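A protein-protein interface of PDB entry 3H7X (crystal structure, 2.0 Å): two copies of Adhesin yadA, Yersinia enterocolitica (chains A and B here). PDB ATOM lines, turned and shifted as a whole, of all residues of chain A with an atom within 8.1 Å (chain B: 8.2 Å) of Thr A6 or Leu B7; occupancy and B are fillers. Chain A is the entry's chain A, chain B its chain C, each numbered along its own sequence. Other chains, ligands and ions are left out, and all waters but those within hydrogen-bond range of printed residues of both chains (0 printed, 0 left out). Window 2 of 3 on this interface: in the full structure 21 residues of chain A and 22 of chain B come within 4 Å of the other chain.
Thr A9 touches Leu B7, but with the chains exchanged Leu A7 does not touch Thr B9 (10.4 Å).
Ala A10 touches its own counterpart, Ala B10.
Ala A10 touches Asn B11, but with the chains exchanged Asn A11 does not touch Ala B10 (6.4 Å).
Tyr A13 touches Asn B11, but with the chains exchanged Asn A11 does not touch Tyr B13 (9.4 Å).
Of the 7 pairs that touch across the chains among the printed residues, 1 has its exchanged pair printed and touching as well.
Printed residues of chain A that touch a printed residue of chain B: Thr A6, Thr A9, Ala A10 and Tyr A13.
Printed residues of chain B that touch a printed residue of chain A: Leu B7, Ala B10, Asn B11 and Thr B14.
Hydrophobic or aromatic side chains of chain B within 4 Å of the printed part of chain A: Leu B7 and Ala B10.
Along chain B the printed residues that touch a printed residue of chain A span positions 7 to 14.
The backbone carbonyl oxygen of Ala B10 sits at hydrogen-bond distance from the side-chain hydroxyl of Thr B14.
Among the printed residues, pairs that only touch across the chains: Tyr A13 with Asn B11, Thr A9 with Leu B7, Thr A6 with Leu B7, Ala A10 with Leu B7, Ala A10 with Asn B11, Ala A10 with Ala B10 and Tyr A13 with Thr B14.
No residue of chain B comes within 4 Å of His A5.
Thr A6 touches one residue of chain B.
Of the printed residues of chain B, Thr A9 touches Leu B7 (3.0 Å).
Of the printed residues of chain B, Tyr A13 touches Asn B11 and Thr B14.
Of the printed residues of chain A, Asn B11 touches Ala A10 and Tyr A13.
Printed residues of chain A within 4 Å of Thr B14: Tyr A13.
The nearest residue of chain A that does not touch Leu B7 is Leu A7 (5.4 Å).
The nearest printed residue of chain B that does not touch Thr A9 is Asn B11 (4.4 Å).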
ATOM      1  N   SER A   3      20.250   7.199 -24.837  1.00  0.00           N
ATOM      2  CA  SER A   3      20.783   6.249 -23.868  1.00  0.00           C
ATOM      3  C   SER A   3      19.738   5.204 -23.487  1.00  0.00           C
ATOM      4  O   SER A   3      19.831   3.991 -23.728  1.00  0.00           O
ATOM      5  CB  SER A   3      21.278   6.978 -22.617  1.00  0.00           C
ATOM      6  OG  SER A   3      20.203   7.595 -21.930  1.00  0.00           O
ATOM      7  N   SER A   4      18.570   5.871 -23.148  1.00  0.00           N
ATOM      8  CA  SER A   4      17.583   5.082 -22.421  1.00  0.00           C
ATOM      9  C   SER A   4      18.177   4.497 -21.143  1.00  0.00           C
ATOM     10  O   SER A   4      19.231   5.288 -20.733  1.00  0.00           O
ATOM     11  CB  SER A   4      17.033   3.962 -23.307  1.00  0.00           C
ATOM     12  OG  SER A   4      18.045   3.025 -23.628  1.00  0.00           O
ATOM     13  N   HIS A   5      18.044   3.424 -20.966  1.00  0.00           N
ATOM     14  CA  HIS A   5      18.394   2.711 -19.744  1.00  0.00           C
ATOM     15  C   HIS A   5      19.870   2.884 -19.407  1.00  0.00           C
ATOM     16  O   HIS A   5      20.158   2.402 -18.247  1.00  0.00           O
ATOM     17  CB  HIS A   5      18.055   1.224 -19.876  1.00  0.00           C
ATOM     18  N   THR A   6      20.802   3.440 -20.113  1.00  0.00           N
ATOM     19  CA  THR A   6      21.989   3.719 -19.330  1.00  0.00           C
ATOM     20  C   THR A   6      21.975   5.046 -18.506  1.00  0.00           C
ATOM     21  O   THR A   6      22.958   5.729 -18.274  1.00  0.00           O
ATOM     22  CB  THR A   6      23.255   2.977 -19.731  1.00  0.00           C
ATOM     23  OG1 THR A   6      23.050   2.308 -21.000  1.00  0.00           O
ATOM     24  CG2 THR A   6      23.393   1.837 -18.726  1.00  0.00           C
ATOM     25  N   LEU A   7      20.766   5.379 -18.080  1.00  0.00           N
ATOM     26  CA  LEU A   7      20.509   6.191 -16.893  1.00  0.00           C
ATOM     27  C   LEU A   7      21.002   5.487 -15.681  1.00  0.00           C
ATOM     28  O   LEU A   7      21.380   6.187 -14.717  1.00  0.00           O
ATOM     29  CB  LEU A   7      18.994   6.348 -16.678  1.00  0.00           C
ATOM     30  CG  LEU A   7      18.413   7.196 -17.792  1.00  0.00           C
ATOM     31  CD1 LEU A   7      17.140   6.557 -18.348  1.00  0.00           C
ATOM     32  CD2 LEU A   7      18.169   8.603 -17.323  1.00  0.00           C
ATOM     33  N   LYS A   8      20.914   4.140 -15.693  1.00  0.00           N
ATOM     34  CA  LYS A   8      21.487   3.266 -14.637  1.00  0.00           C
ATOM     35  C   LYS A   8      22.985   3.374 -14.383  1.00  0.00           C
ATOM     36  O   LYS A   8      23.465   3.221 -13.247  1.00  0.00           O
ATOM     37  CB  LYS A   8      21.217   1.807 -14.975  1.00  0.00           C
ATOM     38  CG  LYS A   8      19.939   1.242 -14.371  1.00  0.00           C
ATOM     39  CD  LYS A   8      20.098  -0.295 -14.300  1.00  0.00           C
ATOM     40  CE  LYS A   8      18.736  -1.030 -14.462  1.00  0.00           C
ATOM     41  NZ  LYS A   8      18.917  -2.560 -14.218  1.00  0.00           N
ATOM     42  N   THR A   9      23.749   3.510 -15.455  1.00  0.00           N
ATOM     43  CA  THR A   9      25.164   3.649 -15.288  1.00  0.00           C
ATOM     44  C   THR A   9      25.486   5.049 -14.842  1.00  0.00           C
ATOM     45  O   THR A   9      26.399   5.225 -14.077  1.00  0.00           O
ATOM     46  CB  THR A   9      25.914   3.285 -16.590  1.00  0.00           C
ATOM     47  OG1 THR A   9      25.723   1.886 -16.808  1.00  0.00           O
ATOM     48  CG2 THR A   9      27.430   3.571 -16.495  1.00  0.00           C
ATOM     49  N   ALA A  10      24.775   6.042 -15.348  1.00  0.00           N
ATOM     50  CA  ALA A  10      24.951   7.428 -14.920  1.00  0.00           C
ATOM     51  C   ALA A  10      24.504   7.620 -13.466  1.00  0.00           C
ATOM     52  O   ALA A  10      25.201   8.229 -12.665  1.00  0.00           O
ATOM     53  CB  ALA A  10      24.193   8.311 -15.786  1.00  0.00           C
ATOM     54  N   ASN A  11      23.312   7.100 -13.147  1.00  0.00           N
ATOM     55  CA  ASN A  11      22.776   7.134 -11.806  1.00  0.00           C
ATOM     56  C   ASN A  11      23.666   6.432 -10.767  1.00  0.00           C
ATOM     57  O   ASN A  11      23.738   6.833  -9.572  1.00  0.00           O
ATOM     58  CB  ASN A  11      21.400   6.483 -11.833  1.00  0.00           C
ATOM     59  CG  ASN A  11      20.288   7.416 -12.344  1.00  0.00           C
ATOM     60  OD1 ASN A  11      20.499   8.542 -12.884  1.00  0.00           O
ATOM     61  ND2 ASN A  11      19.060   6.944 -12.154  1.00  0.00           N
ATOM     62  N   SER A  12      24.335   5.371 -11.191  1.00  0.00           N
ATOM     63  CA  SER A  12      25.166   4.585 -10.305  1.00  0.00           C
ATOM     64  C   SER A  12      26.536   5.182 -10.093  1.00  0.00           C
ATOM     65  O   SER A  12      27.192   4.978  -9.022  1.00  0.00           O
ATOM     66  CB  SER A  12      25.275   3.169 -10.855  1.00  0.00           C
ATOM     67  OG  SER A  12      26.537   2.586 -10.541  1.00  0.00           O
ATOM     68  N   TYR A  13      26.951   5.979 -11.072  1.00  0.00           N
ATOM     69  CA  TYR A  13      28.160   6.765 -10.942  1.00  0.00           C
ATOM     70  C   TYR A  13      27.822   7.918  -9.992  1.00  0.00           C
ATOM     71  O   TYR A  13      28.589   8.220  -9.093  1.00  0.00           O
ATOM     72  CB  TYR A  13      28.601   7.291 -12.292  1.00  0.00           C
ATOM     73  CG  TYR A  13      29.798   8.219 -12.245  1.00  0.00           C
ATOM     74  CD1 TYR A  13      31.060   7.748 -11.916  1.00  0.00           C
ATOM     75  CD2 TYR A  13      29.640   9.558 -12.466  1.00  0.00           C
ATOM     76  CE1 TYR A  13      32.161   8.605 -11.853  1.00  0.00           C
ATOM     77  CE2 TYR A  13      30.739  10.423 -12.422  1.00  0.00           C
ATOM     78  CZ  TYR A  13      31.988   9.934 -12.114  1.00  0.00           C
ATOM     79  OH  TYR A  13      33.034  10.856 -12.083  1.00  0.00           O
ATOM     80  N   THR B   6      25.953   8.768 -23.933  1.00  0.00           N
ATOM     81  CA  THR B   6      26.429   9.981 -23.179  1.00  0.00           C
ATOM     82  C   THR B   6      26.202   9.950 -21.666  1.00  0.00           C
ATOM     83  O   THR B   6      25.590  10.843 -21.053  1.00  0.00           O
ATOM     84  CB  THR B   6      26.134  11.292 -23.861  1.00  0.00           C
ATOM     85  OG1 THR B   6      27.326  12.085 -23.745  1.00  0.00           O
ATOM     86  CG2 THR B   6      24.926  11.979 -23.290  1.00  0.00           C
ATOM     87  N   LEU B   7      26.705   8.863 -21.126  1.00  0.00           N
ATOM     88  CA  LEU B   7      27.025   8.643 -19.745  1.00  0.00           C
ATOM     89  C   LEU B   7      28.047   9.696 -19.387  1.00  0.00           C
ATOM     90  O   LEU B   7      27.914  10.357 -18.359  1.00  0.00           O
ATOM     91  CB  LEU B   7      27.624   7.248 -19.590  1.00  0.00           C
ATOM     92  CG  LEU B   7      26.571   6.149 -19.766  1.00  0.00           C
ATOM     93  CD1 LEU B   7      27.006   4.977 -20.671  1.00  0.00           C
ATOM     94  CD2 LEU B   7      26.154   5.663 -18.388  1.00  0.00           C
ATOM     95  N   LYS B   8      29.017   9.875 -20.284  1.00  0.00           N
ATOM     96  CA  LYS B   8      30.017  10.926 -20.216  1.00  0.00           C
ATOM     97  C   LYS B   8      29.507  12.344 -19.873  1.00  0.00           C
ATOM     98  O   LYS B   8      30.088  13.047 -19.034  1.00  0.00           O
ATOM     99  CB  LYS B   8      30.800  10.967 -21.535  1.00  0.00           C
ATOM    100  CG  LYS B   8      32.014  10.029 -21.615  1.00  0.00           C
ATOM    101  CD  LYS B   8      33.013  10.673 -22.611  1.00  0.00           C
ATOM    102  CE  LYS B   8      33.938   9.687 -23.260  1.00  0.00           C
ATOM    103  NZ  LYS B   8      34.790  10.422 -24.292  1.00  0.00           N
ATOM    104  N   THR B   9      28.458  12.787 -20.551  1.00  0.00           N
ATOM    105  CA  THR B   9      27.869  14.081 -20.233  1.00  0.00           C
ATOM    106  C   THR B   9      27.081  14.044 -18.892  1.00  0.00           C
ATOM    107  O   THR B   9      27.039  15.024 -18.181  1.00  0.00           O
ATOM    108  CB  THR B   9      26.948  14.571 -21.361  1.00  0.00           C
ATOM    109  OG1 THR B   9      27.735  14.870 -22.521  1.00  0.00           O
ATOM    110  CG2 THR B   9      26.218  15.854 -20.982  1.00  0.00           C
ATOM    111  N   ALA B  10      26.485  12.919 -18.556  1.00  0.00           N
ATOM    112  CA  ALA B  10      25.799  12.845 -17.297  1.00  0.00           C
ATOM    113  C   ALA B  10      26.821  12.771 -16.149  1.00  0.00           C
ATOM    114  O   ALA B  10      26.714  13.542 -15.204  1.00  0.00           O
ATOM    115  CB  ALA B  10      24.887  11.671 -17.287  1.00  0.00           C
ATOM    116  N   ASN B  11      27.796  11.870 -16.287  1.00  0.00           N
ATOM    117  CA  ASN B  11      28.890  11.674 -15.379  1.00  0.00           C
ATOM    118  C   ASN B  11      29.705  12.947 -15.083  1.00  0.00           C
ATOM    119  O   ASN B  11      30.093  13.201 -13.937  1.00  0.00           O
ATOM    120  CB  ASN B  11      29.801  10.547 -15.897  1.00  0.00           C
ATOM    121  CG  ASN B  11      29.311   9.238 -15.504  1.00  0.00           C
ATOM    122  OD1 ASN B  11      28.185   9.106 -15.015  1.00  0.00           O
ATOM    123  ND2 ASN B  11      30.121   8.222 -15.703  1.00  0.00           N
ATOM    124  N   SER B  12      29.896  13.783 -16.102  1.00  0.00           N
ATOM    125  CA  SER B  12      30.685  15.004 -15.964  1.00  0.00           C
ATOM    126  C   SER B  12      29.847  16.156 -15.351  1.00  0.00           C
ATOM    127  O   SER B  12      30.369  17.095 -14.824  1.00  0.00           O
ATOM    128  CB  SER B  12      31.286  15.340 -17.330  1.00  0.00           C
ATOM    129  OG  SER B  12      31.154  16.679 -17.594  1.00  0.00           O
ATOM    130  N   TYR B  13      28.530  16.044 -15.399  1.00  0.00           N
ATOM    131  CA  TYR B  13      27.618  16.942 -14.680  1.00  0.00           C
ATOM    132  C   TYR B  13      27.567  16.582 -13.214  1.00  0.00           C
ATOM    133  O   TYR B  13      27.489  17.445 -12.382  1.00  0.00           O
ATOM    134  CB  TYR B  13      26.215  16.843 -15.233  1.00  0.00           C
ATOM    135  CG  TYR B  13      25.221  17.696 -14.490  1.00  0.00           C
ATOM    136  CD1 TYR B  13      25.135  19.070 -14.724  1.00  0.00           C
ATOM    137  CD2 TYR B  13      24.326  17.097 -13.554  1.00  0.00           C
ATOM    138  CE1 TYR B  13      24.215  19.862 -14.045  1.00  0.00           C
ATOM    139  CE2 TYR B  13      23.409  17.855 -12.872  1.00  0.00           C
ATOM    140  CZ  TYR B  13      23.327  19.231 -13.114  1.00  0.00           C
ATOM    141  OH  TYR B  13      22.372  19.997 -12.408  1.00  0.00           O
ATOM    142  N   THR B  14      27.591  15.297 -12.929  1.00  0.00           N
ATOM    143  CA  THR B  14      27.730  14.728 -11.621  1.00  0.00           C
ATOM    144  C   THR B  14      29.032  15.301 -10.956  1.00  0.00           C
ATOM    145  O   THR B  14      28.985  15.913  -9.850  1.00  0.00           O
ATOM    146  CB  THR B  14      27.680  13.149 -11.701  1.00  0.00           C
ATOM    147  OG1 THR B  14      26.309  12.710 -11.884  1.00  0.00           O
ATOM    148  CG2 THR B  14      28.228  12.407 -10.437  1.00  0.00           C
